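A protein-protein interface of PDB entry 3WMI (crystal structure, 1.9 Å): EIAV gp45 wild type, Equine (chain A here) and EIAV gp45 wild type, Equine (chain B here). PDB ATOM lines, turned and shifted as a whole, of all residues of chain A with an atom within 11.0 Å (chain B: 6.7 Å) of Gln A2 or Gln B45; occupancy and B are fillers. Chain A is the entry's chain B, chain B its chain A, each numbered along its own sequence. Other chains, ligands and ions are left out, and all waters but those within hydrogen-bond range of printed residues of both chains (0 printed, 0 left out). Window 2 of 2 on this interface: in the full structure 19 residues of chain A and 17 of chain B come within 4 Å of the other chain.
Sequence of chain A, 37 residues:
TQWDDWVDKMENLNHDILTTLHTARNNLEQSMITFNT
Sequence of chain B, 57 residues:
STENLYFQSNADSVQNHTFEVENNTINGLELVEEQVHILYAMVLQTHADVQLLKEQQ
OE1 of Gln B45 touches NE2 of Gln A2, at 3.5 Å.
CZ2 of Trp A3 touches CE of Met B42 (3.5 Å).
Trp A3 touches Thr B46 (CH2 to OG1, 3.8 Å).
Trp A6 touches Ala B41 (CZ2 to CB, 3.7 Å).
Trp A6 touches Met B42 (CE3 to CG, 3.4 Å).
Trp A6 touches Gln B45.
Hydrophobic or aromatic side chains of chain B within 4 Å of the printed part of chain A: Ala B41 and Met B42.
Along chain B the printed residues that touch a printed residue of chain A span positions 41 to 46.
Among the printed residues, 6 pairs touch across the chains.
Gln A2 touches one residue of chain B.
Gln B45 touches just these residues of chain A: Gln A2 and Trp A6.
Ala B41 touches just one residue of chain A: Trp A6 (3.7 Å).
Thr B46 touches just one residue of chain A: Trp A3 (3.8 Å).
No residue of chain A comes within 4 Å of Ala B48.
No residue of chain A comes within 4 Å of Asp B49.
Of the printed residues of chain B, Trp A3 touches Met B42 (3.5 Å) and Thr B46 (3.8 Å).
Of the printed residues of chain A, Met B42 touches Trp A3 (3.5 Å) and Trp A6 (3.4 Å).
The nearest printed residue of chain A that does not touch Met B42 is Val A7 (4.4 Å).
The side-chain amide nitrogen of Gln B45 is in hydrogen-bond range of the side-chain carboxylate of Asp B49, 3.4 Å away.
O of Met B42 is in hydrogen-bond range of OG1 of Thr B46.
OG1 of Thr A1 lies close to N of Trp A3.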
ATOM      1  N   THR A   1     -13.164 -12.924 -28.627  1.00  0.00           N
ATOM      2  CA  THR A   1     -11.743 -12.851 -28.313  1.00  0.00           C
ATOM      3  C   THR A   1     -11.446 -11.676 -27.398  1.00  0.00           C
ATOM      4  O   THR A   1     -12.287 -10.795 -27.184  1.00  0.00           O
ATOM      5  CB  THR A   1     -10.852 -12.667 -29.565  1.00  0.00           C
ATOM      6  OG1 THR A   1     -11.088 -11.374 -30.151  1.00  0.00           O
ATOM      7  CG2 THR A   1     -11.093 -13.767 -30.592  1.00  0.00           C
ATOM      8  N   GLN A   2     -10.227 -11.671 -26.880  1.00  0.00           N
ATOM      9  CA  GLN A   2      -9.739 -10.593 -26.047  1.00  0.00           C
ATOM     10  C   GLN A   2      -9.902  -9.247 -26.741  1.00  0.00           C
ATOM     11  O   GLN A   2     -10.397  -8.292 -26.142  1.00  0.00           O
ATOM     12  CB  GLN A   2      -8.273 -10.835 -25.740  1.00  0.00           C
ATOM     13  CG  GLN A   2      -7.627  -9.775 -24.895  1.00  0.00           C
ATOM     14  CD  GLN A   2      -6.198 -10.126 -24.574  1.00  0.00           C
ATOM     15  OE1 GLN A   2      -5.815 -10.197 -23.408  1.00  0.00           O
ATOM     16  NE2 GLN A   2      -5.395 -10.360 -25.615  1.00  0.00           N
ATOM     17  N   TRP A   3      -9.487  -9.182 -28.004  1.00  0.00           N
ATOM     18  CA  TRP A   3      -9.488  -7.930 -28.752  1.00  0.00           C
ATOM     19  C   TRP A   3     -10.913  -7.457 -29.043  1.00  0.00           C
ATOM     20  O   TRP A   3     -11.232  -6.288 -28.856  1.00  0.00           O
ATOM     21  CB  TRP A   3      -8.688  -8.071 -30.050  1.00  0.00           C
ATOM     22  CG  TRP A   3      -8.366  -6.762 -30.697  1.00  0.00           C
ATOM     23  CD1 TRP A   3      -9.080  -6.135 -31.679  1.00  0.00           C
ATOM     24  CD2 TRP A   3      -7.255  -5.906 -30.402  1.00  0.00           C
ATOM     25  NE1 TRP A   3      -8.483  -4.945 -32.012  1.00  0.00           N
ATOM     26  CE2 TRP A   3      -7.360  -4.779 -31.242  1.00  0.00           C
ATOM     27  CE3 TRP A   3      -6.179  -5.987 -29.516  1.00  0.00           C
ATOM     28  CZ2 TRP A   3      -6.427  -3.733 -31.220  1.00  0.00           C
ATOM     29  CZ3 TRP A   3      -5.251  -4.949 -29.495  1.00  0.00           C
ATOM     30  CH2 TRP A   3      -5.382  -3.839 -30.343  1.00  0.00           C
ATOM     31  N   ASP A   4     -11.772  -8.371 -29.487  1.00  0.00           N
ATOM     32  CA  ASP A   4     -13.173  -8.032 -29.766  1.00  0.00           C
ATOM     33  C   ASP A   4     -13.861  -7.488 -28.521  1.00  0.00           C
ATOM     34  O   ASP A   4     -14.696  -6.577 -28.606  1.00  0.00           O
ATOM     35  CB  ASP A   4     -13.950  -9.252 -30.268  1.00  0.00           C
ATOM     36  CG  ASP A   4     -13.518  -9.698 -31.650  1.00  0.00           C
ATOM     37  OD1 ASP A   4     -13.081  -8.850 -32.458  1.00  0.00           O
ATOM     38  OD2 ASP A   4     -13.627 -10.907 -31.931  1.00  0.00           O
ATOM     39  N   ASP A   5     -13.517  -8.045 -27.368  1.00  0.00           N
ATOM     40  CA  ASP A   5     -14.162  -7.634 -26.129  1.00  0.00           C
ATOM     41  C   ASP A   5     -13.730  -6.220 -25.754  1.00  0.00           C
ATOM     42  O   ASP A   5     -14.536  -5.433 -25.257  1.00  0.00           O
ATOM     43  CB  ASP A   5     -13.858  -8.603 -24.992  1.00  0.00           C
ATOM     44  CG  ASP A   5     -14.617  -9.921 -25.119  1.00  0.00           C
ATOM     45  OD1 ASP A   5     -15.549 -10.020 -25.947  1.00  0.00           O
ATOM     46  OD2 ASP A   5     -14.278 -10.856 -24.372  1.00  0.00           O
ATOM     47  N   TRP A   6     -12.465  -5.896 -26.007  1.00  0.00           N
ATOM     48  CA  TRP A   6     -11.959  -4.536 -25.779  1.00  0.00           C
ATOM     49  C   TRP A   6     -12.673  -3.539 -26.686  1.00  0.00           C
ATOM     50  O   TRP A   6     -13.075  -2.467 -26.240  1.00  0.00           O
ATOM     51  CB  TRP A   6     -10.448  -4.465 -26.032  1.00  0.00           C
ATOM     52  CG  TRP A   6      -9.583  -5.018 -24.933  1.00  0.00           C
ATOM     53  CD1 TRP A   6      -9.876  -5.071 -23.598  1.00  0.00           C
ATOM     54  CD2 TRP A   6      -8.270  -5.582 -25.076  1.00  0.00           C
ATOM     55  NE1 TRP A   6      -8.829  -5.633 -22.906  1.00  0.00           N
ATOM     56  CE2 TRP A   6      -7.832  -5.959 -23.789  1.00  0.00           C
ATOM     57  CE3 TRP A   6      -7.424  -5.811 -26.170  1.00  0.00           C
ATOM     58  CZ2 TRP A   6      -6.590  -6.557 -23.562  1.00  0.00           C
ATOM     59  CZ3 TRP A   6      -6.180  -6.404 -25.943  1.00  0.00           C
ATOM     60  CH2 TRP A   6      -5.777  -6.764 -24.647  1.00  0.00           C
ATOM     61  N   VAL A   7     -12.817  -3.899 -27.960  1.00  0.00           N
ATOM     62  CA  VAL A   7     -13.536  -3.084 -28.938  1.00  0.00           C
ATOM     63  C   VAL A   7     -14.969  -2.811 -28.489  1.00  0.00           C
ATOM     64  O   VAL A   7     -15.431  -1.673 -28.522  1.00  0.00           O
ATOM     65  CB  VAL A   7     -13.534  -3.754 -30.335  1.00  0.00           C
ATOM     66  CG1 VAL A   7     -14.537  -3.091 -31.250  1.00  0.00           C
ATOM     67  CG2 VAL A   7     -12.147  -3.677 -30.944  1.00  0.00           C
ATOM     68  N   ASP A   8     -15.662  -3.854 -28.052  1.00  0.00           N
ATOM     69  CA  ASP A   8     -17.034  -3.701 -27.554  1.00  0.00           C
ATOM     70  C   ASP A   8     -17.136  -2.758 -26.356  1.00  0.00           C
ATOM     71  O   ASP A   8     -18.048  -1.932 -26.275  1.00  0.00           O
ATOM     72  CB  ASP A   8     -17.617  -5.067 -27.200  1.00  0.00           C
ATOM     73  CG  ASP A   8     -17.923  -5.893 -28.429  1.00  0.00           C
ATOM     74  OD1 ASP A   8     -17.875  -5.328 -29.540  1.00  0.00           O
ATOM     75  OD2 ASP A   8     -18.220  -7.092 -28.293  1.00  0.00           O
ATOM     76  N   LYS A   9     -16.195  -2.878 -25.426  1.00  0.00           N
ATOM     77  CA  LYS A   9     -16.191  -2.019 -24.236  1.00  0.00           C
ATOM     78  C   LYS A   9     -15.895  -0.564 -24.609  1.00  0.00           C
ATOM     79  O   LYS A   9     -16.546   0.370 -24.115  1.00  0.00           O
ATOM     80  CB  LYS A   9     -15.182  -2.542 -23.207  1.00  0.00           C
ATOM     81  CG  LYS A   9     -15.484  -3.955 -22.710  1.00  0.00           C
ATOM     82  CD  LYS A   9     -14.406  -4.475 -21.739  1.00  0.00           C
ATOM     83  CE  LYS A   9     -14.961  -4.684 -20.379  1.00  0.00           C
ATOM     84  NZ  LYS A   9     -14.173  -5.708 -19.642  1.00  0.00           N
ATOM     85  N   MET A  10     -14.923  -0.377 -25.497  1.00  0.00           N
ATOM     86  CA  MET A  10     -14.577   0.958 -25.972  1.00  0.00           C
ATOM     87  C   MET A  10     -15.788   1.615 -26.623  1.00  0.00           C
ATOM     88  O   MET A  10     -16.079   2.788 -26.382  1.00  0.00           O
ATOM     89  CB  MET A  10     -13.399   0.900 -26.958  1.00  0.00           C
ATOM     90  CG  MET A  10     -13.028   2.246 -27.573  1.00  0.00           C
ATOM     91  SD  MET A  10     -12.411   3.418 -26.340  1.00  0.00           S
ATOM     92  CE  MET A  10     -11.275   2.361 -25.472  1.00  0.00           C
ATOM     93  N   TYR B  40      -4.643   1.222 -22.942  1.00  0.00           N
ATOM     94  CA  TYR B  40      -3.372   0.836 -22.338  1.00  0.00           C
ATOM     95  C   TYR B  40      -3.139  -0.669 -22.503  1.00  0.00           C
ATOM     96  O   TYR B  40      -2.061  -1.096 -22.920  1.00  0.00           O
ATOM     97  CB  TYR B  40      -3.360   1.265 -20.863  1.00  0.00           C
ATOM     98  CG  TYR B  40      -2.116   0.910 -20.067  1.00  0.00           C
ATOM     99  CD1 TYR B  40      -0.845   1.201 -20.540  1.00  0.00           C
ATOM    100  CD2 TYR B  40      -2.228   0.339 -18.806  1.00  0.00           C
ATOM    101  CE1 TYR B  40       0.295   0.892 -19.779  1.00  0.00           C
ATOM    102  CE2 TYR B  40      -1.113   0.023 -18.055  1.00  0.00           C
ATOM    103  CZ  TYR B  40       0.139   0.309 -18.540  1.00  0.00           C
ATOM    104  OH  TYR B  40       1.229  -0.011 -17.766  1.00  0.00           O
ATOM    105  N   ALA B  41      -4.156  -1.468 -22.189  1.00  0.00           N
ATOM    106  CA  ALA B  41      -4.065  -2.917 -22.373  1.00  0.00           C
ATOM    107  C   ALA B  41      -3.860  -3.310 -23.835  1.00  0.00           C
ATOM    108  O   ALA B  41      -3.063  -4.202 -24.125  1.00  0.00           O
ATOM    109  CB  ALA B  41      -5.298  -3.609 -21.817  1.00  0.00           C
ATOM    110  N   MET B  42      -4.583  -2.664 -24.749  1.00  0.00           N
ATOM    111  CA  MET B  42      -4.425  -2.944 -26.174  1.00  0.00           C
ATOM    112  C   MET B  42      -3.003  -2.636 -26.600  1.00  0.00           C
ATOM    113  O   MET B  42      -2.398  -3.389 -27.355  1.00  0.00           O
ATOM    114  CB  MET B  42      -5.406  -2.121 -27.019  1.00  0.00           C
ATOM    115  CG  MET B  42      -6.870  -2.472 -26.775  1.00  0.00           C
ATOM    116  SD  MET B  42      -8.014  -1.269 -27.468  1.00  0.00           S
ATOM    117  CE  MET B  42      -8.492  -2.072 -28.990  1.00  0.00           C
ATOM    118  N   VAL B  43      -2.478  -1.523 -26.102  1.00  0.00           N
ATOM    119  CA  VAL B  43      -1.135  -1.059 -26.448  1.00  0.00           C
ATOM    120  C   VAL B  43      -0.060  -2.026 -25.929  1.00  0.00           C
ATOM    121  O   VAL B  43       0.897  -2.359 -26.643  1.00  0.00           O
ATOM    122  CB  VAL B  43      -0.903   0.398 -25.931  1.00  0.00           C
ATOM    123  CG1 VAL B  43       0.592   0.735 -25.846  1.00  0.00           C
ATOM    124  CG2 VAL B  43      -1.629   1.397 -26.838  1.00  0.00           C
ATOM    125  N   LEU B  44      -0.229  -2.488 -24.692  1.00  0.00           N
ATOM    126  CA  LEU B  44       0.677  -3.474 -24.109  1.00  0.00           C
ATOM    127  C   LEU B  44       0.637  -4.805 -24.869  1.00  0.00           C
ATOM    128  O   LEU B  44       1.678  -5.432 -25.104  1.00  0.00           O
ATOM    129  CB  LEU B  44       0.339  -3.702 -22.629  1.00  0.00           C
ATOM    130  CG  LEU B  44       0.673  -2.583 -21.639  1.00  0.00           C
ATOM    131  CD1 LEU B  44       0.206  -2.940 -20.220  1.00  0.00           C
ATOM    132  CD2 LEU B  44       2.151  -2.245 -21.619  1.00  0.00           C
ATOM    133  N   GLN B  45      -0.559  -5.244 -25.240  1.00  0.00           N
ATOM    134  CA  GLN B  45      -0.701  -6.484 -26.004  1.00  0.00           C
ATOM    135  C   GLN B  45      -0.031  -6.390 -27.374  1.00  0.00           C
ATOM    136  O   GLN B  45       0.681  -7.302 -27.791  1.00  0.00           O
ATOM    137  CB  GLN B  45      -2.177  -6.853 -26.167  1.00  0.00           C
ATOM    138  CG  GLN B  45      -2.419  -8.089 -27.035  1.00  0.00           C
ATOM    139  CD  GLN B  45      -1.921  -9.354 -26.379  1.00  0.00           C
ATOM    140  OE1 GLN B  45      -1.994  -9.494 -25.163  1.00  0.00           O
ATOM    141  NE2 GLN B  45      -1.397 -10.281 -27.183  1.00  0.00           N
ATOM    142  N   THR B  46      -0.261  -5.281 -28.070  1.00  0.00           N
ATOM    143  CA  THR B  46       0.352  -5.063 -29.378  1.00  0.00           C
ATOM    144  C   THR B  46       1.874  -5.038 -29.269  1.00  0.00           C
ATOM    145  O   THR B  46       2.577  -5.600 -30.109  1.00  0.00           O
ATOM    146  CB  THR B  46      -0.148  -3.756 -30.021  1.00  0.00           C
ATOM    147  OG1 THR B  46      -1.564  -3.841 -30.220  1.00  0.00           O
ATOM    148  CG2 THR B  46       0.524  -3.528 -31.366  1.00  0.00           C
ATOM    149  N   HIS B  47       2.373  -4.404 -28.215  1.00  0.00           N
ATOM    150  CA  HIS B  47       3.811  -4.343 -27.949  1.00  0.00           C
ATOM    151  C   HIS B  47       4.396  -5.743 -27.799  1.00  0.00           C
ATOM    152  O   HIS B  47       5.453  -6.052 -28.358  1.00  0.00           O
ATOM    153  CB  HIS B  47       4.060  -3.548 -26.666  1.00  0.00           C
ATOM    154  CG  HIS B  47       5.508  -3.427 -26.290  1.00  0.00           C
ATOM    155  ND1 HIS B  47       6.430  -2.775 -27.078  1.00  0.00           N
ATOM    156  CD2 HIS B  47       6.185  -3.861 -25.199  1.00  0.00           C
ATOM    157  CE1 HIS B  47       7.614  -2.813 -26.489  1.00  0.00           C
ATOM    158  NE2 HIS B  47       7.491  -3.465 -25.348  1.00  0.00           N
ATOM    159  N   ALA B  48       3.708  -6.581 -27.033  1.00  0.00           N
ATOM    160  CA  ALA B  48       4.102  -7.983 -26.871  1.00  0.00           C
ATOM    161  C   ALA B  48       4.198  -8.689 -28.218  1.00  0.00           C
ATOM    162  O   ALA B  48       5.187  -9.384 -28.502  1.00  0.00           O
ATOM    163  CB  ALA B  48       3.116  -8.708 -25.969  1.00  0.00           C
ATOM    164  N   ASP B  49       3.175  -8.528 -29.052  1.00  0.00           N
ATOM    165  CA  ASP B  49       3.185  -9.164 -30.369  1.00  0.00           C
ATOM    166  C   ASP B  49       4.369  -8.666 -31.187  1.00  0.00           C
ATOM    167  O   ASP B  49       5.063  -9.449 -31.861  1.00  0.00           O
ATOM    168  CB  ASP B  49       1.885  -8.892 -31.132  1.00  0.00           C
ATOM    169  CG  ASP B  49       0.682  -9.550 -30.491  1.00  0.00           C
ATOM    170  OD1 ASP B  49       0.860 -10.560 -29.769  1.00  0.00           O
ATOM    171  OD2 ASP B  49      -0.440  -9.045 -30.702  1.00  0.00           O
ATOM    172  N   VAL B  50       4.590  -7.361 -31.141  1.00  0.00           N
ATOM    173  CA  VAL B  50       5.690  -6.751 -31.878  1.00  0.00           C
ATOM    174  C   VAL B  50       7.052  -7.267 -31.392  1.00  0.00           C
ATOM    175  O   VAL B  50       7.929  -7.589 -32.194  1.00  0.00           O
ATOM    176  CB  VAL B  50       5.613  -5.213 -31.821  1.00  0.00           C
ATOM    177  CG1 VAL B  50       6.907  -4.594 -32.294  1.00  0.00           C
ATOM    178  CG2 VAL B  50       4.434  -4.719 -32.662  1.00  0.00           C
